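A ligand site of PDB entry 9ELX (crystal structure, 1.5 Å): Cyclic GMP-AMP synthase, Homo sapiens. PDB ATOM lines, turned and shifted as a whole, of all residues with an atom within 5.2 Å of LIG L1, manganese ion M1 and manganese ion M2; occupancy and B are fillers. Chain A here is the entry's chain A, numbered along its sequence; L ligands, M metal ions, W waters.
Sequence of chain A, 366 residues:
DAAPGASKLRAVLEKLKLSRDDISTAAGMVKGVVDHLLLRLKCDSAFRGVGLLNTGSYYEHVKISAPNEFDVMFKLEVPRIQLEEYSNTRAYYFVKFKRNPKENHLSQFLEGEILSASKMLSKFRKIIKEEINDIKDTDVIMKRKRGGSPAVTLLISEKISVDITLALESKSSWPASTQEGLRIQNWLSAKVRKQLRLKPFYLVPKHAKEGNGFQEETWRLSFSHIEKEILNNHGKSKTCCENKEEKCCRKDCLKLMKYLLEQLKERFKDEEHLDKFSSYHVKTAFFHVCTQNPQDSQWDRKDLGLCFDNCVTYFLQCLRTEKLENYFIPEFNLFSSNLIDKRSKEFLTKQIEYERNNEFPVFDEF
Ser 57 touches manganese ion M2.
The nearest printed residue that does not touch manganese ion M2 is Gly 56 (4.8 Å).
CA of Gly 56 touches O5 of LIG L1, at 3.5 Å.
CD of Lys 63 touches O1 of LIG L1, 3.99 Å away.
Tyr 280 touches LIG L1 (CE2 to N5, 3.3 Å).
Of the 22 residues printed, 12 come within 4 Å of LIG L1.
The nearest printed residue that does not touch LIG L1 is Glu 262 (4.1 Å).
Within 4 Å of manganese ion M1: Glu 69, Asp 71 and Asp 163.
Manganese ion M2 is bound by the side-chain carboxylate (OE1) of Glu 69 (2.1 Å), an oxygen (O3) of LIG L1 (2.2 Å), an oxygen (O5) of LIG L1 (2.2 Å), the side-chain carboxylate (OD2) of Asp 71 (2.2 Å), an oxygen (O7) of LIG L1 (2.2 Å) and water W13 (2.3 Å).
Manganese ion M2 has six donor atoms within binding distance.
The side-chain hydroxyl (OH) of Tyr 280 lies within hydrogen-bond range of the side-chain carboxylate (OE2) of Glu 227, 2.6 Å away.
The backbone carbonyl oxygen (O) of Phe 70 is in hydrogen-bond range of the backbone NH (N) of Asp 163, 2.9 Å away.
NZ of Lys 283 lies within salt-bridge range of OE1 of Glu 227 (2.8 Å).
The side-chain amino group (NZ) of Lys 283 lies within salt-bridge range of the side-chain carboxylate (OE1) of Glu 60 (2.7 Å).
The backbone NH (N) of Arg 220 lies close to the backbone carbonyl oxygen (O) of Lys 206, at 3.5 Å.
O of Ser 57 lies within hydrogen-bond range of N of Val 62 (2.9 Å).
The backbone NH (N) of Thr 55 is in hydrogen-bond range of the backbone carbonyl oxygen (O) of Asp 71 (3.1 Å).
The backbone NH (N) of Lys 63 lies within hydrogen-bond range of the backbone carbonyl oxygen (O) of Ser 57 (3.1 Å).
Water W10 lies within hydrogen-bond range of the side-chain carboxylate (OE2) of Glu 262 (2.6 Å), an oxygen (O2) of LIG L1 (2.7 Å) and the side-chain amino group (NZ) of Lys 258 (3.1 Å).
Water W3 lies within hydrogen-bond range of O4 of LIG L1, OG of Ser 279 and N of Tyr 280.
Water W9 lies within hydrogen-bond range of O1 of LIG L1 (2.8 Å), NZ of Lys 63 (2.9 Å) and OE2 of Glu 262 (3.0 Å).
Water W4 bridges O6 of LIG L1 (2.9 Å) and N1 of LG2 L2 (2.9 Å).
Water W7 lies within hydrogen-bond range of N5 of LIG L1 (3.0 Å), NH1 of Arg 220 (3.1 Å) and ND2 of Asn 326 (3.1 Å).
Water W11 bridges the guanidinium group (NH2) of Arg 220 (2.7 Å) and a nitrogen (N4) of LIG L1 (3.2 Å).
The backbone NH (N) of Ser 57 lies close to an oxygen (O5) of LIG L1, 2.8 Å away.
The side-chain carboxylate (OE1) of Glu 227 sits at hydrogen-bond distance from an oxygen (O12) of LIG L1 (2.7 Å).
N5 of LIG L1 lies within hydrogen-bond range of NH1 of Arg 220 (3.5 Å).
NZ of Lys 258 lies within salt-bridge range of O1 of LIG L1.
An oxygen (O12) of LIG L1 sits at hydrogen-bond distance from the side-chain hydroxyl (OG) of Ser 224 (2.9 Å).
OG of Ser 57 lies within hydrogen-bond range of O1 of LIG L1.
The side-chain amino group of Lys 206 is in hydrogen-bond range of an oxygen (O4) of LG2 L2 (3.0 Å).
OG of Ser 279 sits at hydrogen-bond distance from N1 of LIG L1, at 3.1 Å.
The side-chain amino group (NZ) of Lys 283 lies within hydrogen-bond range of an oxygen (O11) of LIG L1 (2.9 Å).
Manganese ion M1 is bound by OE2 of Glu 69 (2.1 Å), OD2 of Asp 163 (2.1 Å), OD1 of Asp 71 (2.1 Å), O1 of LG2 L2 (2.2 Å), O7 of LIG L1 (2.2 Å) and N3 of LG2 L2 (2.3 Å).
Manganese ion M1 has six donor atoms within binding distance.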
ATOM      1  N   THR A  55      -4.250 -32.806 -16.136  1.00  0.00           N
ATOM      2  CA  THR A  55      -4.568 -31.716 -17.079  1.00  0.00           C
ATOM      3  C   THR A  55      -3.682 -31.831 -18.295  1.00  0.00           C
ATOM      4  O   THR A  55      -2.789 -32.672 -18.406  1.00  0.00           O
ATOM      5  CB  THR A  55      -4.339 -30.321 -16.450  1.00  0.00           C
ATOM      6  OG1 THR A  55      -2.947 -30.176 -16.144  1.00  0.00           O
ATOM      7  CG2 THR A  55      -5.125 -30.177 -15.148  1.00  0.00           C
ATOM      8  N   GLY A  56      -3.942 -30.981 -19.274  1.00  0.00           N
ATOM      9  CA  GLY A  56      -3.009 -30.919 -20.406  1.00  0.00           C
ATOM     10  C   GLY A  56      -3.202 -31.996 -21.461  1.00  0.00           C
ATOM     11  O   GLY A  56      -4.110 -32.834 -21.361  1.00  0.00           O
ATOM     12  N   SER A  57      -2.297 -32.010 -22.458  1.00  0.00           N
ATOM     13  CA  SER A  57      -2.617 -32.720 -23.691  1.00  0.00           C
ATOM     14  C   SER A  57      -2.677 -34.233 -23.521  1.00  0.00           C
ATOM     15  O   SER A  57      -3.408 -34.903 -24.262  1.00  0.00           O
ATOM     16  CB  SER A  57      -1.630 -32.362 -24.766  1.00  0.00           C
ATOM     17  OG  SER A  57      -0.300 -32.794 -24.420  1.00  0.00           O
ATOM     18  N   TYR A  58      -1.894 -34.828 -22.629  1.00  0.00           N
ATOM     19  CA  TYR A  58      -1.964 -36.269 -22.480  1.00  0.00           C
ATOM     20  C   TYR A  58      -3.352 -36.681 -22.031  1.00  0.00           C
ATOM     21  O   TYR A  58      -3.942 -37.606 -22.582  1.00  0.00           O
ATOM     22  CB  TYR A  58      -0.922 -36.716 -21.445  1.00  0.00           C
ATOM     23  CG  TYR A  58      -0.944 -38.213 -21.255  1.00  0.00           C
ATOM     24  CD1 TYR A  58      -0.215 -39.016 -22.142  1.00  0.00           C
ATOM     25  CD2 TYR A  58      -1.733 -38.804 -20.255  1.00  0.00           C
ATOM     26  CE1 TYR A  58      -0.238 -40.380 -21.999  1.00  0.00           C
ATOM     27  CE2 TYR A  58      -1.762 -40.191 -20.129  1.00  0.00           C
ATOM     28  CZ  TYR A  58      -0.988 -40.947 -20.999  1.00  0.00           C
ATOM     29  OH  TYR A  58      -1.012 -42.326 -20.875  1.00  0.00           O
ATOM     30  N   GLU A  60      -6.087 -35.000 -22.353  1.00  0.00           N
ATOM     31  CA  GLU A  60      -7.071 -34.691 -23.387  1.00  0.00           C
ATOM     32  C   GLU A  60      -6.900 -35.513 -24.642  1.00  0.00           C
ATOM     33  O   GLU A  60      -7.602 -35.289 -25.635  1.00  0.00           O
ATOM     34  CB  GLU A  60      -7.022 -33.170 -23.730  1.00  0.00           C
ATOM     35  CG  GLU A  60      -6.820 -32.359 -22.449  1.00  0.00           C
ATOM     36  CD  GLU A  60      -6.395 -30.857 -22.675  1.00  0.00           C
ATOM     37  OE1 GLU A  60      -6.983 -29.918 -22.058  1.00  0.00           O
ATOM     38  OE2 GLU A  60      -5.526 -30.642 -23.568  1.00  0.00           O
ATOM     39  N   VAL A  62      -4.634 -35.401 -26.857  1.00  0.00           N
ATOM     40  CA  VAL A  62      -4.106 -34.702 -28.020  1.00  0.00           C
ATOM     41  C   VAL A  62      -2.595 -34.494 -27.882  1.00  0.00           C
ATOM     42  O   VAL A  62      -2.004 -33.782 -28.669  1.00  0.00           O
ATOM     43  CB  VAL A  62      -4.812 -33.362 -28.279  1.00  0.00           C
ATOM     44  CG1 VAL A  62      -6.283 -33.610 -28.747  1.00  0.00           C
ATOM     45  CG2 VAL A  62      -4.739 -32.428 -27.052  1.00  0.00           C
ATOM     46  N   LYS A  63      -1.959 -35.249 -26.986  1.00  0.00           N
ATOM     47  CA  LYS A  63      -0.498 -35.297 -26.990  1.00  0.00           C
ATOM     48  C   LYS A  63      -0.021 -35.985 -28.271  1.00  0.00           C
ATOM     49  O   LYS A  63      -0.591 -37.025 -28.688  1.00  0.00           O
ATOM     50  CB  LYS A  63      -0.055 -36.109 -25.750  1.00  0.00           C
ATOM     51  CG  LYS A  63       1.504 -36.260 -25.632  1.00  0.00           C
ATOM     52  CD  LYS A  63       2.095 -34.986 -25.033  1.00  0.00           C
ATOM     53  CE  LYS A  63       3.633 -34.970 -25.081  1.00  0.00           C
ATOM     54  NZ  LYS A  63       4.148 -34.814 -26.488  1.00  0.00           N
ATOM     55  N   GLU A  69       5.511 -35.866 -21.817  1.00  0.00           N
ATOM     56  CA  GLU A  69       5.251 -34.607 -21.115  1.00  0.00           C
ATOM     57  C   GLU A  69       3.838 -34.634 -20.571  1.00  0.00           C
ATOM     58  O   GLU A  69       2.842 -34.766 -21.315  1.00  0.00           O
ATOM     59  CB  GLU A  69       5.476 -33.407 -22.041  1.00  0.00           C
ATOM     60  CG  GLU A  69       5.817 -32.090 -21.242  1.00  0.00           C
ATOM     61  CD  GLU A  69       4.600 -31.217 -20.963  1.00  0.00           C
ATOM     62  OE1 GLU A  69       3.462 -31.687 -21.221  1.00  0.00           O
ATOM     63  OE2 GLU A  69       4.794 -30.067 -20.491  1.00  0.00           O
ATOM     64  N   PHE A  70       3.763 -34.600 -19.227  1.00  0.00           N
ATOM     65  CA  PHE A  70       2.519 -34.735 -18.496  1.00  0.00           C
ATOM     66  C   PHE A  70       2.315 -33.504 -17.642  1.00  0.00           C
ATOM     67  O   PHE A  70       3.271 -32.969 -17.110  1.00  0.00           O
ATOM     68  CB  PHE A  70       2.537 -35.963 -17.592  1.00  0.00           C
ATOM     69  CG  PHE A  70       2.554 -37.274 -18.321  1.00  0.00           C
ATOM     70  CD1 PHE A  70       3.716 -37.714 -18.945  1.00  0.00           C
ATOM     71  CD2 PHE A  70       1.429 -38.097 -18.309  1.00  0.00           C
ATOM     72  CE1 PHE A  70       3.746 -38.930 -19.567  1.00  0.00           C
ATOM     73  CE2 PHE A  70       1.475 -39.367 -18.923  1.00  0.00           C
ATOM     74  CZ  PHE A  70       2.627 -39.751 -19.587  1.00  0.00           C
ATOM     75  N   ASP A  71       1.051 -33.143 -17.433  1.00  0.00           N
ATOM     76  CA  ASP A  71       0.704 -31.981 -16.641  1.00  0.00           C
ATOM     77  C   ASP A  71      -0.292 -32.370 -15.573  1.00  0.00           C
ATOM     78  O   ASP A  71      -1.223 -33.117 -15.854  1.00  0.00           O
ATOM     79  CB  ASP A  71       0.101 -30.890 -17.518  1.00  0.00           C
ATOM     80  CG  ASP A  71       1.016 -30.535 -18.636  1.00  0.00           C
ATOM     81  OD1 ASP A  71       2.080 -29.922 -18.406  1.00  0.00           O
ATOM     82  OD2 ASP A  71       0.703 -30.917 -19.791  1.00  0.00           O
ATOM     83  N   ASP A 163       4.974 -31.561 -15.290  1.00  0.00           N
ATOM     84  CA  ASP A 163       4.775 -30.226 -14.732  1.00  0.00           C
ATOM     85  C   ASP A 163       3.737 -30.342 -13.652  1.00  0.00           C
ATOM     86  O   ASP A 163       2.604 -30.752 -13.945  1.00  0.00           O
ATOM     87  CB  ASP A 163       4.290 -29.240 -15.802  1.00  0.00           C
ATOM     88  CG  ASP A 163       5.336 -28.921 -16.777  1.00  0.00           C
ATOM     89  OD1 ASP A 163       6.422 -28.429 -16.444  1.00  0.00           O
ATOM     90  OD2 ASP A 163       5.048 -28.954 -17.983  1.00  0.00           O
ATOM     91  N   LYS A 206       1.092 -18.020 -11.058  1.00  0.00           N
ATOM     92  CA  LYS A 206       1.650 -17.286 -12.189  1.00  0.00           C
ATOM     93  C   LYS A 206       1.332 -15.826 -11.946  1.00  0.00           C
ATOM     94  O   LYS A 206       0.161 -15.464 -11.752  1.00  0.00           O
ATOM     95  CB  LYS A 206       1.041 -17.788 -13.509  1.00  0.00           C
ATOM     96  CG  LYS A 206       1.657 -17.117 -14.736  1.00  0.00           C
ATOM     97  CD  LYS A 206       0.901 -17.519 -15.978  1.00  0.00           C
ATOM     98  CE  LYS A 206       1.494 -16.903 -17.259  1.00  0.00           C
ATOM     99  NZ  LYS A 206       2.928 -17.187 -17.413  1.00  0.00           N
ATOM    100  N   ARG A 220      -3.053 -16.445 -10.865  1.00  0.00           N
ATOM    101  CA  ARG A 220      -3.677 -16.434 -12.181  1.00  0.00           C
ATOM    102  C   ARG A 220      -4.856 -17.394 -12.190  1.00  0.00           C
ATOM    103  O   ARG A 220      -4.754 -18.518 -11.706  1.00  0.00           O
ATOM    104  CB  ARG A 220      -2.657 -16.833 -13.255  1.00  0.00           C
ATOM    105  CG  ARG A 220      -3.315 -17.319 -14.520  1.00  0.00           C
ATOM    106  CD  ARG A 220      -3.816 -16.161 -15.355  1.00  0.00           C
ATOM    107  NE  ARG A 220      -2.761 -15.762 -16.253  1.00  0.00           N
ATOM    108  CZ  ARG A 220      -2.632 -16.208 -17.502  1.00  0.00           C
ATOM    109  NH1 ARG A 220      -3.451 -17.118 -17.993  1.00  0.00           N
ATOM    110  NH2 ARG A 220      -1.613 -15.756 -18.237  1.00  0.00           N
ATOM    111  N   SER A 222      -7.262 -20.159 -13.561  1.00  0.00           N
ATOM    112  CA  SER A 222      -7.041 -21.306 -14.413  1.00  0.00           C
ATOM    113  C   SER A 222      -8.298 -22.131 -14.500  1.00  0.00           C
ATOM    114  O   SER A 222      -8.934 -22.481 -13.488  1.00  0.00           O
ATOM    115  CB  SER A 222      -5.891 -22.202 -13.917  1.00  0.00           C
ATOM    116  OG  SER A 222      -5.791 -23.342 -14.789  1.00  0.00           O
ATOM    117  N   SER A 224      -8.051 -25.106 -16.549  1.00  0.00           N
ATOM    118  CA  SER A 224      -7.500 -26.256 -17.272  1.00  0.00           C
ATOM    119  C   SER A 224      -8.456 -27.455 -17.186  1.00  0.00           C
ATOM    120  O   SER A 224      -8.580 -28.226 -18.148  1.00  0.00           O
ATOM    121  CB  SER A 224      -6.132 -26.663 -16.688  1.00  0.00           C
ATOM    122  OG  SER A 224      -5.134 -25.684 -16.880  1.00  0.00           O
ATOM    123  N   GLU A 227     -11.115 -27.052 -19.818  1.00  0.00           N
ATOM    124  CA  GLU A 227     -10.546 -27.380 -21.148  1.00  0.00           C
ATOM    125  C   GLU A 227     -10.512 -28.888 -21.397  1.00  0.00           C
ATOM    126  O   GLU A 227     -10.822 -29.358 -22.507  1.00  0.00           O
ATOM    127  CB  GLU A 227      -9.149 -26.762 -21.348  1.00  0.00           C
ATOM    128  CG  GLU A 227      -9.186 -25.248 -21.078  1.00  0.00           C
ATOM    129  CD  GLU A 227      -7.798 -24.600 -21.091  1.00  0.00           C
ATOM    130  OE1 GLU A 227      -6.754 -25.323 -21.226  1.00  0.00           O
ATOM    131  OE2 GLU A 227      -7.755 -23.343 -20.821  1.00  0.00           O
ATOM    132  N   LYS A 258      -0.924 -28.251 -33.456  1.00  0.00           N
ATOM    133  CA  LYS A 258       0.143 -28.348 -32.473  1.00  0.00           C
ATOM    134  C   LYS A 258       1.433 -28.756 -33.153  1.00  0.00           C
ATOM    135  O   LYS A 258       2.504 -28.253 -32.807  1.00  0.00           O
ATOM    136  CB  LYS A 258      -0.236 -29.380 -31.378  1.00  0.00           C
ATOM    137  CG  LYS A 258      -1.360 -28.909 -30.424  1.00  0.00           C
ATOM    138  CD  LYS A 258      -1.900 -30.114 -29.548  1.00  0.00           C
ATOM    139  CE  LYS A 258      -0.761 -30.809 -28.716  1.00  0.00           C
ATOM    140  NZ  LYS A 258      -0.442 -29.855 -27.617  1.00  0.00           N
ATOM    141  N   GLU A 262       4.901 -26.859 -33.212  1.00  0.00           N
ATOM    142  CA  GLU A 262       6.054 -27.572 -32.672  1.00  0.00           C
ATOM    143  C   GLU A 262       7.188 -27.594 -33.699  1.00  0.00           C
ATOM    144  O   GLU A 262       8.352 -27.316 -33.389  1.00  0.00           O
ATOM    145  CB  GLU A 262       5.678 -29.016 -32.245  1.00  0.00           C
ATOM    146  CG  GLU A 262       4.917 -29.174 -30.855  1.00  0.00           C
ATOM    147  CD  GLU A 262       4.735 -30.630 -30.334  1.00  0.00           C
ATOM    148  OE1 GLU A 262       5.553 -31.490 -30.704  1.00  0.00           O
ATOM    149  OE2 GLU A 262       3.790 -30.920 -29.511  1.00  0.00           O
ATOM    150  N   SER A 279       2.004 -23.802 -27.403  1.00  0.00           N
ATOM    151  CA  SER A 279       0.867 -24.634 -27.771  1.00  0.00           C
ATOM    152  C   SER A 279      -0.435 -24.124 -27.206  1.00  0.00           C
ATOM    153  O   SER A 279      -1.487 -24.404 -27.795  1.00  0.00           O
ATOM    154  CB  SER A 279       1.074 -26.102 -27.302  1.00  0.00           C
ATOM    155  OG  SER A 279       1.006 -26.199 -25.892  1.00  0.00           O
ATOM    156  N   TYR A 280      -0.409 -23.351 -26.105  1.00  0.00           N
ATOM    157  CA  TYR A 280      -1.683 -22.803 -25.621  1.00  0.00           C
ATOM    158  C   TYR A 280      -2.282 -21.812 -26.578  1.00  0.00           C
ATOM    159  O   TYR A 280      -3.509 -21.633 -26.590  1.00  0.00           O
ATOM    160  CB  TYR A 280      -1.479 -22.162 -24.241  1.00  0.00           C
ATOM    161  CG  TYR A 280      -2.756 -21.897 -23.538  1.00  0.00           C
ATOM    162  CD1 TYR A 280      -3.542 -22.976 -23.109  1.00  0.00           C
ATOM    163  CD2 TYR A 280      -3.193 -20.597 -23.329  1.00  0.00           C
ATOM    164  CE1 TYR A 280      -4.727 -22.781 -22.490  1.00  0.00           C
ATOM    165  CE2 TYR A 280      -4.411 -20.390 -22.629  1.00  0.00           C
ATOM    166  CZ  TYR A 280      -5.167 -21.489 -22.269  1.00  0.00           C
ATOM    167  OH  TYR A 280      -6.382 -21.265 -21.654  1.00  0.00           O
ATOM    168  N   LYS A 283      -4.155 -24.005 -28.912  1.00  0.00           N
ATOM    169  CA  LYS A 283      -5.314 -24.591 -28.258  1.00  0.00           C
ATOM    170  C   LYS A 283      -6.451 -23.571 -28.130  1.00  0.00           C
ATOM    171  O   LYS A 283      -7.627 -23.876 -28.374  1.00  0.00           O
ATOM    172  CB  LYS A 283      -4.876 -25.108 -26.904  1.00  0.00           C
ATOM    173  CG  LYS A 283      -5.946 -25.966 -26.181  1.00  0.00           C
ATOM    174  CD  LYS A 283      -5.471 -26.220 -24.754  1.00  0.00           C
ATOM    175  CE  LYS A 283      -6.387 -27.322 -24.103  1.00  0.00           C
ATOM    176  NZ  LYS A 283      -5.936 -27.568 -22.701  1.00  0.00           N
ATOM    177  N   ASN A 326      -8.314 -14.989 -24.445  1.00  0.00           N
ATOM    178  CA  ASN A 326      -8.432 -16.176 -23.610  1.00  0.00           C
ATOM    179  C   ASN A 326      -9.861 -16.693 -23.706  1.00  0.00           C
ATOM    180  O   ASN A 326     -10.832 -15.920 -23.695  1.00  0.00           O
ATOM    181  CB  ASN A 326      -8.063 -15.772 -22.182  1.00  0.00           C
ATOM    182  CG  ASN A 326      -8.121 -16.955 -21.207  1.00  0.00           C
ATOM    183  OD1 ASN A 326      -9.210 -17.435 -20.887  1.00  0.00           O
ATOM    184  ND2 ASN A 326      -6.959 -17.459 -20.772  1.00  0.00           N
HETATM  185  P1  LIG L   1       1.732 -30.019 -25.073  1.00  0.00           P
HETATM  186  O1  LIG L   1       1.178 -31.171 -25.780  1.00  0.00           O
HETATM  187  O2  LIG L   1       2.745 -29.229 -25.954  1.00  0.00           O
HETATM  188  O3  LIG L   1       2.337 -30.406 -23.758  1.00  0.00           O
HETATM  189  P2  LIG L   1      -0.398 -28.838 -23.392  1.00  0.00           P
HETATM  190  O4  LIG L   1      -1.781 -28.391 -23.694  1.00  0.00           O
HETATM  191  O5  LIG L   1      -0.293 -30.052 -22.460  1.00  0.00           O
HETATM  192  N1  LIG L   1       0.410 -29.010 -24.833  1.00  0.00           N
HETATM  193  P3  LIG L   1       1.313 -27.328 -21.506  1.00  0.00           P
HETATM  194  O6  LIG L   1       2.150 -26.158 -21.911  1.00  0.00           O
HETATM  195  O7  LIG L   1       2.038 -28.609 -21.120  1.00  0.00           O
HETATM  196  O8  LIG L   1       0.264 -27.608 -22.685  1.00  0.00           O
HETATM  197  O9  LIG L   1       0.350 -26.859 -20.377  1.00  0.00           O
HETATM  198  C1  LIG L   1      -0.521 -27.817 -19.765  1.00  0.00           C
HETATM  199  C2  LIG L   1      -1.880 -27.165 -19.604  1.00  0.00           C
HETATM  200  O10 LIG L   1      -1.716 -26.026 -18.730  1.00  0.00           O
HETATM  201  C3  LIG L   1      -2.515 -26.583 -20.846  1.00  0.00           C
HETATM  202  O11 LIG L   1      -3.268 -27.544 -21.580  1.00  0.00           O
HETATM  203  C4  LIG L   1      -3.452 -25.532 -20.266  1.00  0.00           C
HETATM  204  O12 LIG L   1      -4.620 -26.161 -19.742  1.00  0.00           O
HETATM  205  C5  LIG L   1      -2.608 -24.990 -19.124  1.00  0.00           C
HETATM  206  N2  LIG L   1      -1.824 -23.831 -19.566  1.00  0.00           N
HETATM  207  C6  LIG L   1      -0.582 -23.830 -20.156  1.00  0.00           C
HETATM  208  N3  LIG L   1      -0.177 -22.642 -20.550  1.00  0.00           N
HETATM  209  C7  LIG L   1      -1.215 -21.808 -20.183  1.00  0.00           C
HETATM  210  C8  LIG L   1      -1.414 -20.418 -20.310  1.00  0.00           C
HETATM  211  N4  LIG L   1      -0.501 -19.597 -20.845  1.00  0.00           N
HETATM  212  N5  LIG L   1      -2.583 -19.916 -19.873  1.00  0.00           N
HETATM  213  C9  LIG L   1      -3.475 -20.733 -19.312  1.00  0.00           C
HETATM  214  N6  LIG L   1      -3.408 -22.061 -19.142  1.00  0.00           N
HETATM  215  C10 LIG L   1      -2.246 -22.528 -19.599  1.00  0.00           C
HETATM  216  C1  LG2 L   2       2.683 -21.228 -18.149  1.00  0.00           C
HETATM  217  N1  LG2 L   2       4.150 -22.518 -19.648  1.00  0.00           N
HETATM  218  C2  LG2 L   2       4.990 -23.515 -19.273  1.00  0.00           C
HETATM  219  C3  LG2 L   2       6.101 -24.806 -21.051  1.00  0.00           C
HETATM  220  C4  LG2 L   2       5.536 -27.100 -21.398  1.00  0.00           C
HETATM  221  C5  LG2 L   2       3.318 -25.941 -18.585  1.00  0.00           C
HETATM  222  C6  LG2 L   2      -1.583 -22.938 -15.699  1.00  0.00           C
HETATM  223  C7  LG2 L   2      -0.728 -24.000 -15.792  1.00  0.00           C
HETATM  224  C8  LG2 L   2       0.422 -23.764 -16.522  1.00  0.00           C
HETATM  225  C9  LG2 L   2       0.736 -22.527 -17.122  1.00  0.00           C
HETATM  226  C10 LG2 L   2      -0.151 -21.474 -16.989  1.00  0.00           C
HETATM  227  C11 LG2 L   2      -1.317 -21.722 -16.244  1.00  0.00           C
HETATM  228  C12 LG2 L   2       3.982 -21.282 -18.907  1.00  0.00           C
HETATM  229  C13 LG2 L   2       5.160 -24.721 -20.036  1.00  0.00           C
HETATM  230  C14 LG2 L   2       6.326 -26.000 -21.767  1.00  0.00           C
HETATM  231  C15 LG2 L   2       4.446 -25.896 -19.706  1.00  0.00           C
HETATM  232  F1  LG2 L   2      -2.755 -23.114 -14.965  1.00  0.00           F
HETATM  233  N2  LG2 L   2       1.956 -22.398 -17.835  1.00  0.00           N
HETATM  234  N3  LG2 L   2       4.667 -27.020 -20.372  1.00  0.00           N
HETATM  235  O1  LG2 L   2       2.845 -27.039 -18.353  1.00  0.00           O
HETATM  236  O2  LG2 L   2       2.982 -24.848 -18.115  1.00  0.00           O
HETATM  237  O3  LG2 L   2       5.602 -23.348 -18.221  1.00  0.00           O
HETATM  238  O4  LG2 L   2       2.259 -20.117 -17.790  1.00  0.00           O
HETATM  239 CL1  LG2 L   2      -2.466 -20.465 -16.081  1.00  0.00          CL
HETATM  240 MN    MN M   1       3.525 -28.759 -19.460  1.00  0.00          MN
HETATM  241 MN    MN M   2       1.647 -30.693 -21.740  1.00  0.00          MN
HETATM  242  O   HOH W   1       5.114 -30.698 -24.062  1.00  0.00           O
HETATM  243  O   HOH W   2       0.643 -27.063 -16.698  1.00  0.00           O
HETATM  244  O   HOH W   3      -1.876 -25.906 -24.928  1.00  0.00           O
HETATM  245  O   HOH W   4       2.348 -23.286 -21.788  1.00  0.00           O
HETATM  246  O   HOH W   5      -2.283 -27.801 -27.094  1.00  0.00           O
HETATM  247  O   HOH W   6      -5.376 -23.106 -17.467  1.00  0.00           O
HETATM  248  O   HOH W   7      -3.859 -17.483 -21.028  1.00  0.00           O
HETATM  249  O   HOH W   8      -3.623 -29.628 -25.234  1.00  0.00           O
HETATM  250  O   HOH W   9       2.358 -32.885 -27.724  1.00  0.00           O
HETATM  251  O   HOH W  10       2.304 -29.006 -28.653  1.00  0.00           O
HETATM  252  O   HOH W  11      -0.899 -16.442 -20.731  1.00  0.00           O
HETATM  253  O   HOH W  12       4.301 -27.253 -25.019  1.00  0.00           O
HETATM  254  O   HOH W  13       0.997 -32.833 -22.092  1.00  0.00           O
